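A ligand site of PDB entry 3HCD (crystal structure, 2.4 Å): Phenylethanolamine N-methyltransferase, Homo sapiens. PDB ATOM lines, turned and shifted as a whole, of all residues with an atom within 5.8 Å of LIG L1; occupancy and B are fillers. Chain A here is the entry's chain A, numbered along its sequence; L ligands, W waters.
OH of Tyr 40 sits at hydrogen-bond distance from O1 of LIG L1, at 2.7 Å.
N1 of LIG L1 lies within salt-bridge range of OE2 of Glu 219, 3.3 Å away.
The side-chain amino group of Lys 57 lies within hydrogen-bond range of an oxygen (O1) of LIG L1, at 3.1 Å.
OD2 of Asp 267 lies within hydrogen-bond range of O3 of LIG L1 (3.3 Å).
OH of Tyr 40 lies within hydrogen-bond range of O2 of LG2 L2 (2.5 Å).
OH of Tyr 35 sits at hydrogen-bond distance from O2 of LG2 L2 (2.8 Å).
OH of Tyr 85 is in hydrogen-bond range of O1 of LG2 L2 (2.5 Å).
The side-chain hydroxyl (OH) of Tyr 85 lies close to the side-chain hydroxyl (OH) of Tyr 40 (3.3 Å).
The guanidinium group (NH1) of Arg 44 lies within salt-bridge range of the side-chain carboxylate (OD2) of Asp 267 (2.7 Å).
The side-chain amide oxygen (OD1) of Asn 39 sits at hydrogen-bond distance from the guanidinium group (NH1) of Arg 44 (3.0 Å).
N of Val 269 lies within hydrogen-bond range of OD1 of Asp 267.
The backbone carbonyl oxygen (O) of Tyr 35 sits close to the side-chain amide nitrogen (ND2) of Asn 39, 3.3 Å away.
Asn 39 touches LIG L1.
Arg 44 touches LIG L1.
Val 53 touches LIG L1.
CE1 of Phe 182 touches O1 of LIG L1 (3.5 Å).
CD2 of Tyr 222 touches N1 of LIG L1, at 3.3 Å.
Within 4 Å of LIG L1: Asn 39, Tyr 40, Arg 44, Val 53, Lys 57, Phe 182, Glu 219, Tyr 222 and Asp 267.
The nearest printed residue that does not touch LIG L1 is Val 269 (4.004 Å).
Water W2 lies within hydrogen-bond range of O2 of LIG L1 (2.7 Å), O of Asn 39 (2.7 Å) and NZ of Lys 57 (2.7 Å).
Water W1 lies within hydrogen-bond range of a nitrogen (N1) of LIG L1 (2.7 Å), the side-chain carboxylate (OE2) of Glu 185 (2.9 Å) and the side-chain carboxylate (OE2) of Glu 219 (3.1 Å).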
ATOM      1  N   TYR A  35      14.403  -1.169  20.187  1.00  0.00           N
ATOM      2  CA  TYR A  35      13.372  -0.332  19.612  1.00  0.00           C
ATOM      3  C   TYR A  35      13.861   1.127  19.592  1.00  0.00           C
ATOM      4  O   TYR A  35      13.844   1.769  18.531  1.00  0.00           O
ATOM      5  CB  TYR A  35      12.082  -0.459  20.401  1.00  0.00           C
ATOM      6  CG  TYR A  35      10.982   0.464  19.918  1.00  0.00           C
ATOM      7  CD1 TYR A  35      10.218   0.153  18.801  1.00  0.00           C
ATOM      8  CD2 TYR A  35      10.694   1.656  20.606  1.00  0.00           C
ATOM      9  CE1 TYR A  35       9.182   1.006  18.357  1.00  0.00           C
ATOM     10  CE2 TYR A  35       9.660   2.503  20.183  1.00  0.00           C
ATOM     11  CZ  TYR A  35       8.921   2.184  19.051  1.00  0.00           C
ATOM     12  OH  TYR A  35       7.915   3.030  18.634  1.00  0.00           O
ATOM     13  N   ASN A  39      14.684   3.493  16.119  1.00  0.00           N
ATOM     14  CA  ASN A  39      13.759   4.576  15.784  1.00  0.00           C
ATOM     15  C   ASN A  39      14.081   5.930  16.391  1.00  0.00           C
ATOM     16  O   ASN A  39      13.477   6.951  16.003  1.00  0.00           O
ATOM     17  CB  ASN A  39      12.359   4.196  16.209  1.00  0.00           C
ATOM     18  CG  ASN A  39      11.867   2.974  15.487  1.00  0.00           C
ATOM     19  OD1 ASN A  39      11.843   2.941  14.267  1.00  0.00           O
ATOM     20  ND2 ASN A  39      11.493   1.955  16.248  1.00  0.00           N
ATOM     21  N   TYR A  40      15.025   5.969  17.318  1.00  0.00           N
ATOM     22  CA  TYR A  40      15.328   7.201  18.011  1.00  0.00           C
ATOM     23  C   TYR A  40      16.814   7.491  18.111  1.00  0.00           C
ATOM     24  O   TYR A  40      17.187   8.423  18.788  1.00  0.00           O
ATOM     25  CB  TYR A  40      14.623   7.229  19.369  1.00  0.00           C
ATOM     26  CG  TYR A  40      13.117   7.104  19.172  1.00  0.00           C
ATOM     27  CD1 TYR A  40      12.480   5.882  19.300  1.00  0.00           C
ATOM     28  CD2 TYR A  40      12.368   8.200  18.791  1.00  0.00           C
ATOM     29  CE1 TYR A  40      11.113   5.759  19.090  1.00  0.00           C
ATOM     30  CE2 TYR A  40      11.025   8.097  18.574  1.00  0.00           C
ATOM     31  CZ  TYR A  40      10.397   6.877  18.724  1.00  0.00           C
ATOM     32  OH  TYR A  40       9.056   6.773  18.498  1.00  0.00           O
ATOM     33  N   ARG A  44      17.261   8.123  12.011  1.00  0.00           N
ATOM     34  CA  ARG A  44      15.956   8.698  12.329  1.00  0.00           C
ATOM     35  C   ARG A  44      16.038   9.594  13.542  1.00  0.00           C
ATOM     36  O   ARG A  44      15.205  10.480  13.731  1.00  0.00           O
ATOM     37  CB  ARG A  44      14.886   7.631  12.572  1.00  0.00           C
ATOM     38  CG  ARG A  44      14.691   6.642  11.403  1.00  0.00           C
ATOM     39  CD  ARG A  44      13.494   5.739  11.609  1.00  0.00           C
ATOM     40  NE  ARG A  44      13.157   5.005  10.384  1.00  0.00           N
ATOM     41  CZ  ARG A  44      12.239   4.042  10.313  1.00  0.00           C
ATOM     42  NH1 ARG A  44      11.538   3.676  11.382  1.00  0.00           N
ATOM     43  NH2 ARG A  44      12.023   3.464   9.143  1.00  0.00           N
ATOM     44  N   VAL A  53      11.783  12.760  10.215  1.00  0.00           N
ATOM     45  CA  VAL A  53      10.543  12.383  10.878  1.00  0.00           C
ATOM     46  C   VAL A  53      10.460  12.901  12.308  1.00  0.00           C
ATOM     47  O   VAL A  53       9.374  13.244  12.769  1.00  0.00           O
ATOM     48  CB  VAL A  53      10.367  10.865  10.884  1.00  0.00           C
ATOM     49  CG1 VAL A  53      11.505  10.207  11.653  1.00  0.00           C
ATOM     50  CG2 VAL A  53       8.949  10.472  11.430  1.00  0.00           C
ATOM     51  N   LYS A  57       7.409  15.206  13.767  1.00  0.00           N
ATOM     52  CA  LYS A  57       6.560  14.840  14.887  1.00  0.00           C
ATOM     53  C   LYS A  57       6.610  15.934  15.958  1.00  0.00           C
ATOM     54  O   LYS A  57       5.572  16.350  16.474  1.00  0.00           O
ATOM     55  CB  LYS A  57       7.002  13.473  15.440  1.00  0.00           C
ATOM     56  CG  LYS A  57       6.606  12.260  14.572  1.00  0.00           C
ATOM     57  CD  LYS A  57       6.996  10.907  15.205  1.00  0.00           C
ATOM     58  CE  LYS A  57       8.495  10.854  15.495  1.00  0.00           C
ATOM     59  NZ  LYS A  57       8.996   9.500  15.833  1.00  0.00           N
ATOM     60  N   TYR A  85       9.499  11.596  24.160  1.00  0.00           N
ATOM     61  CA  TYR A  85       9.465  12.728  23.216  1.00  0.00           C
ATOM     62  C   TYR A  85       8.039  13.206  22.953  1.00  0.00           C
ATOM     63  O   TYR A  85       7.799  14.395  22.700  1.00  0.00           O
ATOM     64  CB  TYR A  85      10.134  12.329  21.897  1.00  0.00           C
ATOM     65  CG  TYR A  85       9.243  11.464  21.038  1.00  0.00           C
ATOM     66  CD1 TYR A  85       8.373  12.040  20.115  1.00  0.00           C
ATOM     67  CD2 TYR A  85       9.236  10.069  21.173  1.00  0.00           C
ATOM     68  CE1 TYR A  85       7.518  11.243  19.330  1.00  0.00           C
ATOM     69  CE2 TYR A  85       8.400   9.270  20.371  1.00  0.00           C
ATOM     70  CZ  TYR A  85       7.531   9.870  19.478  1.00  0.00           C
ATOM     71  OH  TYR A  85       6.707   9.085  18.688  1.00  0.00           O
ATOM     72  N   PHE A 182       2.169   5.630  17.916  1.00  0.00           N
ATOM     73  CA  PHE A 182       2.560   4.304  17.422  1.00  0.00           C
ATOM     74  C   PHE A 182       2.091   3.148  18.316  1.00  0.00           C
ATOM     75  O   PHE A 182       2.762   2.124  18.451  1.00  0.00           O
ATOM     76  CB  PHE A 182       4.089   4.229  17.248  1.00  0.00           C
ATOM     77  CG  PHE A 182       4.635   5.291  16.356  1.00  0.00           C
ATOM     78  CD1 PHE A 182       5.356   6.361  16.901  1.00  0.00           C
ATOM     79  CD2 PHE A 182       4.381   5.284  14.995  1.00  0.00           C
ATOM     80  CE1 PHE A 182       5.848   7.352  16.094  1.00  0.00           C
ATOM     81  CE2 PHE A 182       4.872   6.275  14.189  1.00  0.00           C
ATOM     82  CZ  PHE A 182       5.613   7.309  14.740  1.00  0.00           C
ATOM     83  N   GLU A 185      -2.323   0.965  16.090  1.00  0.00           N
ATOM     84  CA  GLU A 185      -2.008   0.222  14.886  1.00  0.00           C
ATOM     85  C   GLU A 185      -0.954  -0.873  15.085  1.00  0.00           C
ATOM     86  O   GLU A 185      -0.892  -1.837  14.324  1.00  0.00           O
ATOM     87  CB  GLU A 185      -1.628   1.160  13.743  1.00  0.00           C
ATOM     88  CG  GLU A 185      -0.205   1.653  13.775  1.00  0.00           C
ATOM     89  CD  GLU A 185      -0.010   2.885  14.641  1.00  0.00           C
ATOM     90  OE1 GLU A 185      -0.974   3.384  15.259  1.00  0.00           O
ATOM     91  OE2 GLU A 185       1.143   3.365  14.690  1.00  0.00           O
ATOM     92  N   ALA A 186      -0.149  -0.739  16.130  1.00  0.00           N
ATOM     93  CA  ALA A 186       0.903  -1.710  16.381  1.00  0.00           C
ATOM     94  C   ALA A 186       0.464  -2.830  17.309  1.00  0.00           C
ATOM     95  O   ALA A 186       1.175  -3.821  17.430  1.00  0.00           O
ATOM     96  CB  ALA A 186       2.147  -1.008  16.955  1.00  0.00           C
ATOM     97  N   ALA A 216       1.916   5.065  12.532  1.00  0.00           N
ATOM     98  CA  ALA A 216       2.576   4.663  11.293  1.00  0.00           C
ATOM     99  C   ALA A 216       1.513   4.483  10.198  1.00  0.00           C
ATOM    100  O   ALA A 216       0.400   4.030  10.483  1.00  0.00           O
ATOM    101  CB  ALA A 216       3.339   3.402  11.525  1.00  0.00           C
ATOM    102  N   GLU A 219       1.979   0.558   7.382  1.00  0.00           N
ATOM    103  CA  GLU A 219       3.097  -0.243   7.890  1.00  0.00           C
ATOM    104  C   GLU A 219       2.566  -1.632   8.225  1.00  0.00           C
ATOM    105  O   GLU A 219       1.429  -1.763   8.656  1.00  0.00           O
ATOM    106  CB  GLU A 219       3.692   0.393   9.155  1.00  0.00           C
ATOM    107  CG  GLU A 219       4.698  -0.497   9.882  1.00  0.00           C
ATOM    108  CD  GLU A 219       5.287   0.161  11.143  1.00  0.00           C
ATOM    109  OE1 GLU A 219       6.386   0.756  11.072  1.00  0.00           O
ATOM    110  OE2 GLU A 219       4.633   0.105  12.211  1.00  0.00           O
ATOM    111  N   TRP A 221       4.933  -4.370   9.602  1.00  0.00           N
ATOM    112  CA  TRP A 221       5.764  -4.981  10.642  1.00  0.00           C
ATOM    113  C   TRP A 221       6.870  -4.015  11.058  1.00  0.00           C
ATOM    114  O   TRP A 221       7.211  -3.122  10.309  1.00  0.00           O
ATOM    115  CB  TRP A 221       6.417  -6.252  10.106  1.00  0.00           C
ATOM    116  CG  TRP A 221       7.232  -5.968   8.903  1.00  0.00           C
ATOM    117  CD1 TRP A 221       6.800  -5.903   7.603  1.00  0.00           C
ATOM    118  CD2 TRP A 221       8.629  -5.670   8.871  1.00  0.00           C
ATOM    119  NE1 TRP A 221       7.849  -5.595   6.773  1.00  0.00           N
ATOM    120  CE2 TRP A 221       8.981  -5.438   7.526  1.00  0.00           C
ATOM    121  CE3 TRP A 221       9.622  -5.559   9.844  1.00  0.00           C
ATOM    122  CZ2 TRP A 221      10.287  -5.110   7.136  1.00  0.00           C
ATOM    123  CZ3 TRP A 221      10.919  -5.209   9.461  1.00  0.00           C
ATOM    124  CH2 TRP A 221      11.236  -5.012   8.111  1.00  0.00           C
ATOM    125  N   TYR A 222       7.430  -4.225  12.251  1.00  0.00           N
ATOM    126  CA  TYR A 222       8.646  -3.546  12.678  1.00  0.00           C
ATOM    127  C   TYR A 222       9.371  -4.418  13.684  1.00  0.00           C
ATOM    128  O   TYR A 222       8.767  -5.273  14.345  1.00  0.00           O
ATOM    129  CB  TYR A 222       8.355  -2.148  13.249  1.00  0.00           C
ATOM    130  CG  TYR A 222       7.702  -2.158  14.599  1.00  0.00           C
ATOM    131  CD1 TYR A 222       8.450  -1.993  15.753  1.00  0.00           C
ATOM    132  CD2 TYR A 222       6.330  -2.323  14.729  1.00  0.00           C
ATOM    133  CE1 TYR A 222       7.860  -2.011  17.005  1.00  0.00           C
ATOM    134  CE2 TYR A 222       5.718  -2.347  15.987  1.00  0.00           C
ATOM    135  CZ  TYR A 222       6.494  -2.193  17.106  1.00  0.00           C
ATOM    136  OH  TYR A 222       5.914  -2.190  18.348  1.00  0.00           O
ATOM    137  N   VAL A 231       1.794  -5.245  12.304  1.00  0.00           N
ATOM    138  CA  VAL A 231       1.153  -3.947  12.361  1.00  0.00           C
ATOM    139  C   VAL A 231       0.007  -3.927  11.368  1.00  0.00           C
ATOM    140  O   VAL A 231       0.159  -4.371  10.243  1.00  0.00           O
ATOM    141  CB  VAL A 231       2.132  -2.809  11.971  1.00  0.00           C
ATOM    142  CG1 VAL A 231       1.451  -1.435  12.085  1.00  0.00           C
ATOM    143  CG2 VAL A 231       3.447  -2.888  12.767  1.00  0.00           C
ATOM    144  N   MET A 258       7.648   8.945   4.466  1.00  0.00           N
ATOM    145  CA  MET A 258       8.962   8.539   4.926  1.00  0.00           C
ATOM    146  C   MET A 258      10.008   8.593   3.776  1.00  0.00           C
ATOM    147  O   MET A 258       9.944   7.813   2.834  1.00  0.00           O
ATOM    148  CB  MET A 258       8.876   7.157   5.556  1.00  0.00           C
ATOM    149  CG  MET A 258      10.104   6.785   6.405  1.00  0.00           C
ATOM    150  SD  MET A 258      10.348   7.698   7.957  1.00  0.00           S
ATOM    151  CE  MET A 258       8.764   7.529   8.730  1.00  0.00           C
ATOM    152  N   VAL A 266      14.460  -1.740   9.538  1.00  0.00           N
ATOM    153  CA  VAL A 266      13.827  -2.023  10.839  1.00  0.00           C
ATOM    154  C   VAL A 266      12.298  -2.122  10.718  1.00  0.00           C
ATOM    155  O   VAL A 266      11.604  -2.438  11.682  1.00  0.00           O
ATOM    156  CB  VAL A 266      14.163  -0.966  11.920  1.00  0.00           C
ATOM    157  CG1 VAL A 266      15.660  -0.794  12.061  1.00  0.00           C
ATOM    158  CG2 VAL A 266      13.494   0.353  11.621  1.00  0.00           C
ATOM    159  N   ASP A 267      11.780  -1.813   9.537  1.00  0.00           N
ATOM    160  CA  ASP A 267      10.333  -1.869   9.337  1.00  0.00           C
ATOM    161  C   ASP A 267       9.990  -1.545   7.905  1.00  0.00           C
ATOM    162  O   ASP A 267      10.885  -1.439   7.068  1.00  0.00           O
ATOM    163  CB  ASP A 267       9.594  -0.925  10.267  1.00  0.00           C
ATOM    164  CG  ASP A 267      10.026   0.560  10.069  1.00  0.00           C
ATOM    165  OD1 ASP A 267      10.269   0.963   8.915  1.00  0.00           O
ATOM    166  OD2 ASP A 267      10.146   1.335  11.054  1.00  0.00           O
ATOM    167  N   VAL A 269       7.433   0.949   7.293  1.00  0.00           N
ATOM    168  CA  VAL A 269       6.574   2.130   7.415  1.00  0.00           C
ATOM    169  C   VAL A 269       6.658   2.975   6.126  1.00  0.00           C
ATOM    170  O   VAL A 269       7.740   3.150   5.578  1.00  0.00           O
ATOM    171  CB  VAL A 269       6.957   2.989   8.641  1.00  0.00           C
ATOM    172  CG1 VAL A 269       8.323   3.651   8.404  1.00  0.00           C
ATOM    173  CG2 VAL A 269       5.906   4.043   8.917  1.00  0.00           C
ATOM    174  N   VAL A 272       4.004   8.617   8.194  1.00  0.00           N
ATOM    175  CA  VAL A 272       3.560   8.822   9.562  1.00  0.00           C
ATOM    176  C   VAL A 272       2.441   9.854   9.569  1.00  0.00           C
ATOM    177  O   VAL A 272       2.506  10.869   8.838  1.00  0.00           O
ATOM    178  CB  VAL A 272       4.725   9.299  10.463  1.00  0.00           C
ATOM    179  CG1 VAL A 272       4.240   9.751  11.806  1.00  0.00           C
ATOM    180  CG2 VAL A 272       5.789   8.214  10.612  1.00  0.00           C
HETATM  181  O1  LIG L   1       9.175   6.410  15.816  1.00  0.00           O
HETATM  182  C1  LIG L   1       8.894   5.618  14.698  1.00  0.00           C
HETATM  183  C2  LIG L   1       8.208   4.410  14.784  1.00  0.00           C
HETATM  184  C3  LIG L   1       9.296   6.088  13.448  1.00  0.00           C
HETATM  185  O2  LIG L   1      10.049   7.244  13.349  1.00  0.00           O
HETATM  186  C4  LIG L   1       9.032   5.385  12.287  1.00  0.00           C
HETATM  187  C5  LIG L   1       8.346   4.176  12.373  1.00  0.00           C
HETATM  188  C6  LIG L   1       7.941   3.684  13.603  1.00  0.00           C
HETATM  189  C7  LIG L   1       7.142   2.369  13.632  1.00  0.00           C
HETATM  190  O3  LIG L   1       7.936   1.221  13.546  1.00  0.00           O
HETATM  191  C8  LIG L   1       6.269   2.324  14.889  1.00  0.00           C
HETATM  192  N1  LIG L   1       5.863   0.963  15.145  1.00  0.00           N
HETATM  193  N1  LG2 L   2       4.748   5.520  22.082  1.00  0.00           N
HETATM  194  C1  LG2 L   2       6.145   5.311  21.768  1.00  0.00           C
HETATM  195  C2  LG2 L   2       6.481   3.828  21.775  1.00  0.00           C
HETATM  196  C3  LG2 L   2       5.448   3.047  20.942  1.00  0.00           C
HETATM  197  S1  LG2 L   2       5.788   1.274  20.632  1.00  0.00           S
HETATM  198  C4  LG2 L   2       6.546   5.881  20.420  1.00  0.00           C
HETATM  199  O1  LG2 L   2       6.042   7.137  20.087  1.00  0.00           O
HETATM  200  O2  LG2 L   2       7.535   5.430  19.998  1.00  0.00           O
HETATM  201  C5  LG2 L   2       4.201   0.472  21.018  1.00  0.00           C
HETATM  202  C6  LG2 L   2       4.055   0.237  22.518  1.00  0.00           C
HETATM  203  O3  LG2 L   2       2.845  -0.428  22.562  1.00  0.00           O
HETATM  204  C7  LG2 L   2       5.074  -0.715  23.180  1.00  0.00           C
HETATM  205  O4  LG2 L   2       5.719  -0.076  24.271  1.00  0.00           O
HETATM  206  C8  LG2 L   2       4.246  -1.750  23.583  1.00  0.00           C
HETATM  207  O5  LG2 L   2       4.614  -2.490  24.722  1.00  0.00           O
HETATM  208  C9  LG2 L   2       2.965  -1.174  23.711  1.00  0.00           C
HETATM  209  N2  LG2 L   2       1.874  -2.128  23.820  1.00  0.00           N
HETATM  210  C10 LG2 L   2       1.883  -3.408  23.429  1.00  0.00           C
HETATM  211  N3  LG2 L   2       0.627  -3.933  23.638  1.00  0.00           N
HETATM  212  C11 LG2 L   2      -0.165  -2.949  24.155  1.00  0.00           C
HETATM  213  C12 LG2 L   2      -1.460  -2.901  24.562  1.00  0.00           C
HETATM  214  N4  LG2 L   2      -2.236  -4.100  24.414  1.00  0.00           N
HETATM  215  N5  LG2 L   2      -2.023  -1.804  25.068  1.00  0.00           N
HETATM  216  C13 LG2 L   2      -1.265  -0.698  25.187  1.00  0.00           C
HETATM  217  N6  LG2 L   2       0.026  -0.745  24.800  1.00  0.00           N
HETATM  218  C14 LG2 L   2       0.584  -1.849  24.284  1.00  0.00           C
HETATM  219  O   HOH W   1       3.179   1.270  14.636  1.00  0.00           O
HETATM  220  O   HOH W   2      11.479   8.572  15.167  1.00  0.00           O
